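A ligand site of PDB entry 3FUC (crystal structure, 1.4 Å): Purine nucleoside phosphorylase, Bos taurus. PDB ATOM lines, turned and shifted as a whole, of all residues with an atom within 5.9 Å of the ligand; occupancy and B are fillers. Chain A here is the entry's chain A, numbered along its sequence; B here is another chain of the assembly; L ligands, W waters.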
ATOM      1  N   CYS A  31      -4.922   1.919 -19.284  1.00  0.00           N
ATOM      2  CA  CYS A  31      -4.244   3.135 -19.739  1.00  0.00           C
ATOM      3  C   CYS A  31      -4.975   4.383 -19.358  1.00  0.00           C
ATOM      4  O   CYS A  31      -6.023   4.691 -19.892  1.00  0.00           O
ATOM      5  CB  CYS A  31      -4.032   3.086 -21.266  1.00  0.00           C
ATOM      6  SG  CYS A  31      -3.075   1.656 -21.821  1.00  0.00           S
ATOM      7  N   GLY A  32      -4.411   5.136 -18.424  1.00  0.00           N
ATOM      8  CA  GLY A  32      -4.954   6.428 -18.092  1.00  0.00           C
ATOM      9  C   GLY A  32      -4.414   7.501 -19.011  1.00  0.00           C
ATOM     10  O   GLY A  32      -3.734   7.204 -20.023  1.00  0.00           O
ATOM     11  N   SER A  33      -4.721   8.746 -18.670  1.00  0.00           N
ATOM     12  CA  SER A  33      -4.368   9.921 -19.493  1.00  0.00           C
ATOM     13  C   SER A  33      -2.887   9.951 -19.775  1.00  0.00           C
ATOM     14  O   SER A  33      -2.072   9.791 -18.864  1.00  0.00           O
ATOM     15  CB  SER A  33      -4.744  11.205 -18.766  1.00  0.00           C
ATOM     16  OG  SER A  33      -6.133  11.245 -18.523  1.00  0.00           O
ATOM     17  N   ARG A  84     -10.985   4.077 -20.047  1.00  0.00           N
ATOM     18  CA  ARG A  84     -11.471   3.400 -18.837  1.00  0.00           C
ATOM     19  C   ARG A  84     -12.767   4.036 -18.396  1.00  0.00           C
ATOM     20  O   ARG A  84     -13.241   4.986 -19.028  1.00  0.00           O
ATOM     21  CB  ARG A  84     -10.408   3.462 -17.720  1.00  0.00           C
ATOM     22  CG  ARG A  84     -10.074   4.887 -17.238  1.00  0.00           C
ATOM     23  CD  ARG A  84     -10.127   5.056 -15.735  1.00  0.00           C
ATOM     24  NE  ARG A  84      -9.160   4.222 -15.022  1.00  0.00           N
ATOM     25  CZ  ARG A  84      -7.856   4.488 -14.923  1.00  0.00           C
ATOM     26  NH1 ARG A  84      -7.325   5.550 -15.531  1.00  0.00           N
ATOM     27  NH2 ARG A  84      -7.056   3.676 -14.246  1.00  0.00           N
ATOM     28  N   HIS A  86     -15.291   5.895 -15.455  1.00  0.00           N
ATOM     29  CA  HIS A  86     -15.144   6.824 -14.321  1.00  0.00           C
ATOM     30  C   HIS A  86     -16.440   7.044 -13.570  1.00  0.00           C
ATOM     31  O   HIS A  86     -17.520   7.161 -14.167  1.00  0.00           O
ATOM     32  CB  HIS A  86     -14.615   8.179 -14.769  1.00  0.00           C
ATOM     33  CG  HIS A  86     -13.352   8.093 -15.553  1.00  0.00           C
ATOM     34  ND1 HIS A  86     -13.343   7.938 -16.916  1.00  0.00           N
ATOM     35  CD2 HIS A  86     -12.056   8.189 -15.163  1.00  0.00           C
ATOM     36  CE1 HIS A  86     -12.093   7.903 -17.330  1.00  0.00           C
ATOM     37  NE2 HIS A  86     -11.291   8.076 -16.296  1.00  0.00           N
ATOM     38  N   TYR A  88     -17.274   9.852 -12.363  1.00  0.00           N
ATOM     39  CA  TYR A  88     -17.830  11.151 -12.773  1.00  0.00           C
ATOM     40  C   TYR A  88     -18.672  11.054 -14.030  1.00  0.00           C
ATOM     41  O   TYR A  88     -19.465  11.934 -14.280  1.00  0.00           O
ATOM     42  CB  TYR A  88     -16.753  12.224 -12.932  1.00  0.00           C
ATOM     43  CG  TYR A  88     -15.747  11.996 -14.030  1.00  0.00           C
ATOM     44  CD1 TYR A  88     -16.085  12.177 -15.373  1.00  0.00           C
ATOM     45  CD2 TYR A  88     -14.420  11.628 -13.731  1.00  0.00           C
ATOM     46  CE1 TYR A  88     -15.134  11.955 -16.389  1.00  0.00           C
ATOM     47  CE2 TYR A  88     -13.495  11.429 -14.724  1.00  0.00           C
ATOM     48  CZ  TYR A  88     -13.853  11.584 -16.053  1.00  0.00           C
ATOM     49  OH  TYR A  88     -12.889  11.369 -17.035  1.00  0.00           O
ATOM     50  N   THR A 114      -2.753   3.297 -14.641  1.00  0.00           N
ATOM     51  CA  THR A 114      -2.203   4.661 -14.641  1.00  0.00           C
ATOM     52  C   THR A 114      -3.301   5.688 -14.725  1.00  0.00           C
ATOM     53  O   THR A 114      -4.465   5.367 -15.024  1.00  0.00           O
ATOM     54  CB  THR A 114      -1.158   4.892 -15.736  1.00  0.00           C
ATOM     55  OG1 THR A 114      -1.820   5.151 -16.970  1.00  0.00           O
ATOM     56  CG2 THR A 114      -0.288   3.658 -15.982  1.00  0.00           C
ATOM     57  N   ASN A 115      -2.919   6.938 -14.468  1.00  0.00           N
ATOM     58  CA  ASN A 115      -3.884   8.021 -14.502  1.00  0.00           C
ATOM     59  C   ASN A 115      -3.143   9.341 -14.669  1.00  0.00           C
ATOM     60  O   ASN A 115      -1.882   9.371 -14.620  1.00  0.00           O
ATOM     61  CB  ASN A 115      -4.727   8.030 -13.225  1.00  0.00           C
ATOM     62  CG  ASN A 115      -3.873   8.138 -11.996  1.00  0.00           C
ATOM     63  OD1 ASN A 115      -3.130   9.088 -11.830  1.00  0.00           O
ATOM     64  ND2 ASN A 115      -4.038   7.182 -11.075  1.00  0.00           N
ATOM     65  N   ALA A 116      -3.908  10.414 -14.893  1.00  0.00           N
ATOM     66  CA  ALA A 116      -3.429  11.793 -14.668  1.00  0.00           C
ATOM     67  C   ALA A 116      -3.876  12.265 -13.285  1.00  0.00           C
ATOM     68  O   ALA A 116      -4.943  11.850 -12.786  1.00  0.00           O
ATOM     69  CB  ALA A 116      -3.999  12.741 -15.697  1.00  0.00           C
ATOM     70  N   ALA A 117      -3.098  13.156 -12.680  1.00  0.00           N
ATOM     71  CA  ALA A 117      -3.428  13.647 -11.357  1.00  0.00           C
ATOM     72  C   ALA A 117      -2.905  15.042 -11.173  1.00  0.00           C
ATOM     73  O   ALA A 117      -1.911  15.451 -11.798  1.00  0.00           O
ATOM     74  CB  ALA A 117      -2.827  12.749 -10.295  1.00  0.00           C
ATOM     75  N   GLY A 118      -3.563  15.800 -10.316  1.00  0.00           N
ATOM     76  CA  GLY A 118      -3.032  17.089  -9.877  1.00  0.00           C
ATOM     77  C   GLY A 118      -1.993  16.915  -8.781  1.00  0.00           C
ATOM     78  O   GLY A 118      -2.137  16.074  -7.882  1.00  0.00           O
ATOM     79  N   GLY A 119      -0.933  17.724  -8.826  1.00  0.00           N
ATOM     80  CA  GLY A 119       0.119  17.641  -7.823  1.00  0.00           C
ATOM     81  C   GLY A 119      -0.253  18.406  -6.569  1.00  0.00           C
ATOM     82  O   GLY A 119      -0.458  19.629  -6.619  1.00  0.00           O
ATOM     83  N   TYR A 192      -1.743   8.628  -3.741  1.00  0.00           N
ATOM     84  CA  TYR A 192      -2.798   9.155  -4.623  1.00  0.00           C
ATOM     85  C   TYR A 192      -4.137   9.153  -3.873  1.00  0.00           C
ATOM     86  O   TYR A 192      -4.535   8.117  -3.314  1.00  0.00           O
ATOM     87  CB  TYR A 192      -2.880   8.258  -5.844  1.00  0.00           C
ATOM     88  CG  TYR A 192      -3.965   8.549  -6.837  1.00  0.00           C
ATOM     89  CD1 TYR A 192      -3.770   9.400  -7.907  1.00  0.00           C
ATOM     90  CD2 TYR A 192      -5.193   7.875  -6.755  1.00  0.00           C
ATOM     91  CE1 TYR A 192      -4.780   9.618  -8.860  1.00  0.00           C
ATOM     92  CE2 TYR A 192      -6.182   8.094  -7.701  1.00  0.00           C
ATOM     93  CZ  TYR A 192      -5.982   8.938  -8.752  1.00  0.00           C
ATOM     94  OH  TYR A 192      -6.974   9.080  -9.694  1.00  0.00           O
ATOM     95  N   LEU A 195     -11.007  11.220  -5.545  1.00  0.00           N
ATOM     96  CA  LEU A 195     -12.323  11.787  -5.264  1.00  0.00           C
ATOM     97  C   LEU A 195     -13.179  11.693  -6.521  1.00  0.00           C
ATOM     98  O   LEU A 195     -12.680  11.356  -7.582  1.00  0.00           O
ATOM     99  CB  LEU A 195     -12.267  13.173  -4.675  1.00  0.00           C
ATOM    100  CG  LEU A 195     -11.175  14.075  -5.193  1.00  0.00           C
ATOM    101  CD1 LEU A 195     -11.329  14.348  -6.677  1.00  0.00           C
ATOM    102  CD2 LEU A 195     -11.181  15.384  -4.382  1.00  0.00           C
ATOM    103  N   GLY A 197     -14.854  13.883  -8.511  1.00  0.00           N
ATOM    104  CA  GLY A 197     -14.871  14.838  -9.632  1.00  0.00           C
ATOM    105  C   GLY A 197     -16.322  15.045 -10.136  1.00  0.00           C
ATOM    106  O   GLY A 197     -17.283  14.593  -9.511  1.00  0.00           O
ATOM    107  N   ASN A 199     -15.423  18.292 -11.187  1.00  0.00           N
ATOM    108  CA  ASN A 199     -14.802  19.607 -11.015  1.00  0.00           C
ATOM    109  C   ASN A 199     -13.408  19.441 -10.390  1.00  0.00           C
ATOM    110  O   ASN A 199     -13.147  18.474  -9.669  1.00  0.00           O
ATOM    111  CB  ASN A 199     -15.636  20.557 -10.130  1.00  0.00           C
ATOM    112  CG  ASN A 199     -15.803  20.033  -8.711  1.00  0.00           C
ATOM    113  OD1 ASN A 199     -16.629  19.160  -8.478  1.00  0.00           O
ATOM    114  ND2 ASN A 199     -14.950  20.486  -7.795  1.00  0.00           N
ATOM    115  N   PHE A 200     -12.516  20.392 -10.688  1.00  0.00           N
ATOM    116  CA  PHE A 200     -11.270  20.503  -9.964  1.00  0.00           C
ATOM    117  C   PHE A 200     -11.492  21.192  -8.604  1.00  0.00           C
ATOM    118  O   PHE A 200     -12.500  21.872  -8.392  1.00  0.00           O
ATOM    119  CB  PHE A 200     -10.238  21.266 -10.808  1.00  0.00           C
ATOM    120  CG  PHE A 200      -9.875  20.607 -12.112  1.00  0.00           C
ATOM    121  CD1 PHE A 200      -9.292  19.353 -12.148  1.00  0.00           C
ATOM    122  CD2 PHE A 200     -10.001  21.313 -13.309  1.00  0.00           C
ATOM    123  CE1 PHE A 200      -8.895  18.746 -13.364  1.00  0.00           C
ATOM    124  CE2 PHE A 200      -9.590  20.727 -14.543  1.00  0.00           C
ATOM    125  CZ  PHE A 200      -9.041  19.432 -14.555  1.00  0.00           C
ATOM    126  N   GLU A 201     -10.531  21.024  -7.714  1.00  0.00           N
ATOM    127  CA  GLU A 201     -10.677  21.391  -6.300  1.00  0.00           C
ATOM    128  C   GLU A 201     -10.597  22.885  -6.020  1.00  0.00           C
ATOM    129  O   GLU A 201      -9.876  23.637  -6.705  1.00  0.00           O
ATOM    130  CB  GLU A 201      -9.578  20.753  -5.482  1.00  0.00           C
ATOM    131  CG  GLU A 201      -9.684  19.235  -5.375  1.00  0.00           C
ATOM    132  CD  GLU A 201      -9.362  18.500  -6.656  1.00  0.00           C
ATOM    133  OE1 GLU A 201      -8.499  18.974  -7.469  1.00  0.00           O
ATOM    134  OE2 GLU A 201      -9.985  17.445  -6.887  1.00  0.00           O
ATOM    135  N   VAL A 217      -3.837  14.086  -6.575  1.00  0.00           N
ATOM    136  CA  VAL A 217      -5.296  13.922  -6.506  1.00  0.00           C
ATOM    137  C   VAL A 217      -5.851  13.614  -7.891  1.00  0.00           C
ATOM    138  O   VAL A 217      -5.457  14.245  -8.878  1.00  0.00           O
ATOM    139  CB  VAL A 217      -5.996  15.160  -5.881  1.00  0.00           C
ATOM    140  CG1 VAL A 217      -5.655  16.472  -6.588  1.00  0.00           C
ATOM    141  CG2 VAL A 217      -7.508  14.934  -5.884  1.00  0.00           C
ATOM    142  N   GLY A 218      -6.750  12.646  -7.956  1.00  0.00           N
ATOM    143  CA  GLY A 218      -7.337  12.292  -9.231  1.00  0.00           C
ATOM    144  C   GLY A 218      -8.720  11.690  -9.080  1.00  0.00           C
ATOM    145  O   GLY A 218      -9.300  11.716  -7.970  1.00  0.00           O
ATOM    146  N   MET A 219      -9.243  11.133 -10.175  1.00  0.00           N
ATOM    147  CA  MET A 219     -10.651  10.730 -10.264  1.00  0.00           C
ATOM    148  C   MET A 219     -10.840   9.287 -10.698  1.00  0.00           C
ATOM    149  O   MET A 219     -11.933   8.917 -11.133  1.00  0.00           O
ATOM    150  CB  MET A 219     -11.380  11.664 -11.253  1.00  0.00           C
ATOM    151  CG  MET A 219     -11.260  13.127 -10.910  1.00  0.00           C
ATOM    152  SD  MET A 219     -12.084  14.174 -12.144  1.00  0.00           S
ATOM    153  CE  MET A 219     -11.579  15.794 -11.599  1.00  0.00           C
ATOM    154  N   SER A 220      -9.818   8.442 -10.596  1.00  0.00           N
ATOM    155  CA  SER A 220      -9.926   7.055 -11.058  1.00  0.00           C
ATOM    156  C   SER A 220      -9.090   6.105 -10.208  1.00  0.00           C
ATOM    157  O   SER A 220      -8.687   6.458  -9.107  1.00  0.00           O
ATOM    158  CB  SER A 220      -9.463   6.981 -12.516  1.00  0.00           C
ATOM    159  OG  SER A 220      -8.056   7.109 -12.575  1.00  0.00           O
ATOM    160  N   THR A 221      -8.832   4.906 -10.731  1.00  0.00           N
ATOM    161  CA  THR A 221      -7.754   3.988 -10.312  1.00  0.00           C
ATOM    162  C   THR A 221      -8.017   3.188  -9.052  1.00  0.00           C
ATOM    163  O   THR A 221      -7.970   1.956  -9.048  1.00  0.00           O
ATOM    164  CB  THR A 221      -6.408   4.756 -10.229  1.00  0.00           C
ATOM    165  OG1 THR A 221      -6.093   5.257 -11.539  1.00  0.00           O
ATOM    166  CG2 THR A 221      -5.271   3.827  -9.855  1.00  0.00           C
ATOM    167  N   THR A 242      -0.126  16.425 -14.093  1.00  0.00           N
ATOM    168  CA  THR A 242      -0.446  17.254 -15.243  1.00  0.00           C
ATOM    169  C   THR A 242      -0.560  18.746 -14.897  1.00  0.00           C
ATOM    170  O   THR A 242      -0.678  19.580 -15.800  1.00  0.00           O
ATOM    171  CB  THR A 242      -1.723  16.809 -15.897  1.00  0.00           C
ATOM    172  OG1 THR A 242      -2.747  16.678 -14.873  1.00  0.00           O
ATOM    173  CG2 THR A 242      -1.555  15.400 -16.436  1.00  0.00           C
ATOM    174  N   ASN A 243      -0.541  19.066 -13.606  1.00  0.00           N
ATOM    175  CA  ASN A 243      -0.746  20.427 -13.113  1.00  0.00           C
ATOM    176  C   ASN A 243      -0.420  20.459 -11.634  1.00  0.00           C
ATOM    177  O   ASN A 243      -0.607  19.444 -10.918  1.00  0.00           O
ATOM    178  CB  ASN A 243      -2.186  20.923 -13.354  1.00  0.00           C
ATOM    179  CG  ASN A 243      -3.242  20.013 -12.744  1.00  0.00           C
ATOM    180  OD1 ASN A 243      -3.379  18.847 -13.133  1.00  0.00           O
ATOM    181  ND2 ASN A 243      -3.994  20.549 -11.784  1.00  0.00           N
ATOM    182  N   VAL A 245      -1.693  21.827  -8.315  1.00  0.00           N
ATOM    183  CA  VAL A 245      -2.991  22.362  -7.875  1.00  0.00           C
ATOM    184  C   VAL A 245      -2.819  23.735  -7.216  1.00  0.00           C
ATOM    185  O   VAL A 245      -1.778  24.018  -6.629  1.00  0.00           O
ATOM    186  CB  VAL A 245      -3.709  21.390  -6.896  1.00  0.00           C
ATOM    187  CG1 VAL A 245      -3.839  19.967  -7.481  1.00  0.00           C
ATOM    188  CG2 VAL A 245      -3.020  21.380  -5.555  1.00  0.00           C
ATOM    189  N   ALA A 255      -6.708  25.451 -12.756  1.00  0.00           N
ATOM    190  CA  ALA A 255      -6.643  24.136 -13.390  1.00  0.00           C
ATOM    191  C   ALA A 255      -7.574  24.079 -14.598  1.00  0.00           C
ATOM    192  O   ALA A 255      -8.677  24.633 -14.584  1.00  0.00           O
ATOM    193  CB  ALA A 255      -7.015  23.032 -12.389  1.00  0.00           C
ATOM    194  N   VAL A 260      -3.927  19.872 -19.003  1.00  0.00           N
ATOM    195  CA  VAL A 260      -3.851  18.450 -18.689  1.00  0.00           C
ATOM    196  C   VAL A 260      -3.583  17.638 -19.965  1.00  0.00           C
ATOM    197  O   VAL A 260      -2.704  16.767 -19.982  1.00  0.00           O
ATOM    198  CB  VAL A 260      -5.135  17.956 -17.944  1.00  0.00           C
ATOM    199  CG1 VAL A 260      -5.140  16.423 -17.760  1.00  0.00           C
ATOM    200  CG2 VAL A 260      -5.259  18.684 -16.606  1.00  0.00           C
ATOM    201  N   PHE B 159     -14.479  19.318 -16.986  1.00  0.00           N
ATOM    202  CA  PHE B 159     -13.740  19.438 -15.725  1.00  0.00           C
ATOM    203  C   PHE B 159     -13.636  20.913 -15.325  1.00  0.00           C
ATOM    204  O   PHE B 159     -12.575  21.529 -15.505  1.00  0.00           O
ATOM    205  CB  PHE B 159     -12.340  18.838 -15.869  1.00  0.00           C
ATOM    206  CG  PHE B 159     -12.321  17.410 -16.319  1.00  0.00           C
ATOM    207  CD1 PHE B 159     -12.688  16.379 -15.466  1.00  0.00           C
ATOM    208  CD2 PHE B 159     -11.867  17.091 -17.608  1.00  0.00           C
ATOM    209  CE1 PHE B 159     -12.626  15.046 -15.896  1.00  0.00           C
ATOM    210  CE2 PHE B 159     -11.800  15.756 -18.025  1.00  0.00           C
ATOM    211  CZ  PHE B 159     -12.198  14.744 -17.178  1.00  0.00           C
HETATM  212  O1  LIG L   1      -6.417   9.527 -16.521  1.00  0.00           O
HETATM  213  P1  LIG L   1      -7.749   9.174 -15.769  1.00  0.00           P
HETATM  214  O2  LIG L   1      -7.438   8.909 -14.214  1.00  0.00           O
HETATM  215  O3  LIG L   1      -8.493   8.019 -16.362  1.00  0.00           O
HETATM  216  C1  LIG L   1      -8.868  10.614 -15.759  1.00  0.00           C
HETATM  217  F1  LIG L   1      -9.398  10.749 -17.005  1.00  0.00           F
HETATM  218  F2  LIG L   1      -9.866  10.387 -14.906  1.00  0.00           F
HETATM  219  C2  LIG L   1      -8.109  11.887 -15.406  1.00  0.00           C
HETATM  220  C3  LIG L   1      -9.110  13.005 -15.023  1.00  0.00           C
HETATM  221  C4  LIG L   1      -8.377  14.305 -14.630  1.00  0.00           C
HETATM  222  C5  LIG L   1      -7.286  14.027 -13.575  1.00  0.00           C
HETATM  223  C6  LIG L   1      -6.705  15.320 -12.993  1.00  0.00           C
HETATM  224  C7  LIG L   1      -5.736  16.096 -13.522  1.00  0.00           C
HETATM  225  N1  LIG L   1      -5.534  17.144 -12.694  1.00  0.00           N
HETATM  226  C8  LIG L   1      -6.351  17.077 -11.622  1.00  0.00           C
HETATM  227  C9  LIG L   1      -7.103  15.917 -11.810  1.00  0.00           C
HETATM  228  N2  LIG L   1      -8.114  15.458 -10.894  1.00  0.00           N
HETATM  229  C10 LIG L   1      -8.295  16.184  -9.893  1.00  0.00           C
HETATM  230  N3  LIG L   1      -9.179  15.895  -8.907  1.00  0.00           N
HETATM  231  N4  LIG L   1      -7.609  17.411  -9.593  1.00  0.00           N
HETATM  232  C11 LIG L   1      -6.597  17.870 -10.509  1.00  0.00           C
HETATM  233  O4  LIG L   1      -6.005  18.925 -10.248  1.00  0.00           O
HETATM  234  O   HOH W   1     -10.810  11.797 -19.794  1.00  0.00           O
HETATM  235  O   HOH W   2      -7.097  10.457 -12.083  1.00  0.00           O
HETATM  236  O   HOH W   3      -7.091  20.997  -8.770  1.00  0.00           O
HETATM  237  O   HOH W   4      -8.415   7.742 -19.110  1.00  0.00           O
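The backbone NH of Gly 118 lies close to a nitrogen (N1) of the ligand (3.4 Å).
The guanidinium group (NH1) of Arg 84 is in salt-bridge range of an oxygen (O3) of the ligand (2.9 Å).
N of Ala 116 is in hydrogen-bond range of O1 of the ligand (3.1 Å).
OE2 of Glu 201 sits at hydrogen-bond distance from N3 of the ligand, at 2.7 Å.
The side-chain hydroxyl of Ser 33 lies within hydrogen-bond range of an oxygen (O1) of the ligand.
The side-chain hydroxyl (OG) of Ser 220 sits at hydrogen-bond distance from an oxygen (O2) of the ligand (2.5 Å).
OD1 of Asn 243 sits at hydrogen-bond distance from N1 of the ligand (2.8 Å).
The backbone NH of Ser 33 is in hydrogen-bond range of an oxygen (O1) of the ligand, 2.8 Å away.
NE2 of His 86 lies within hydrogen-bond range of O3 of the ligand (2.8 Å).
OG1 of Thr 221 lies within hydrogen-bond range of NH2 of Arg 84 (3.3 Å).
O of Gly 119 lies within hydrogen-bond range of N of Val 245, at 3.0 Å.
N of Gly 119 lies within hydrogen-bond range of O of Asn 243 (2.7 Å).
The side-chain hydroxyl (OH) of Tyr 88 lies within hydrogen-bond range of a ring nitrogen (ND1) of His 86 (3.5 Å).
N of Leu 195 lies within hydrogen-bond range of O of Gly 218, 3.0 Å away.
N of Ser 220 sits at hydrogen-bond distance from OH of Tyr 192 (3.1 Å).
The side-chain amide nitrogen of Asn 115 lies within hydrogen-bond range of the side-chain hydroxyl of Thr 221.
The backbone NH (N) of Gly 32 is in hydrogen-bond range of the side-chain hydroxyl (OG1) of Thr 114, at 3.0 Å.
Merely in contact with the ligand: Asn 115, Thr 242, Leu 195, Phe 200, Tyr 88, Val 217, Met 219, Gly 218, Val 245, Ala 117 and Gly 32.
19 residues have an atom within 4 Å of the ligand: Gly 32, Ser 33, Arg 84, His 86, Tyr 88, Asn 115, Ala 116, Ala 117, Gly 118, Leu 195, Phe 200, Glu 201, Val 217, Gly 218, Met 219, Ser 220, Thr 242, Asn 243 and Val 245.
Water W2 lies within hydrogen-bond range of O2 of the ligand (2.7 Å), O of Ala 116 (2.7 Å), OH of Tyr 192 (2.8 Å) and N of Met 219 (3.0 Å).
Water W3 lies within hydrogen-bond range of O4 of the ligand (2.8 Å) and OE1 of Glu 201 (2.8 Å).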
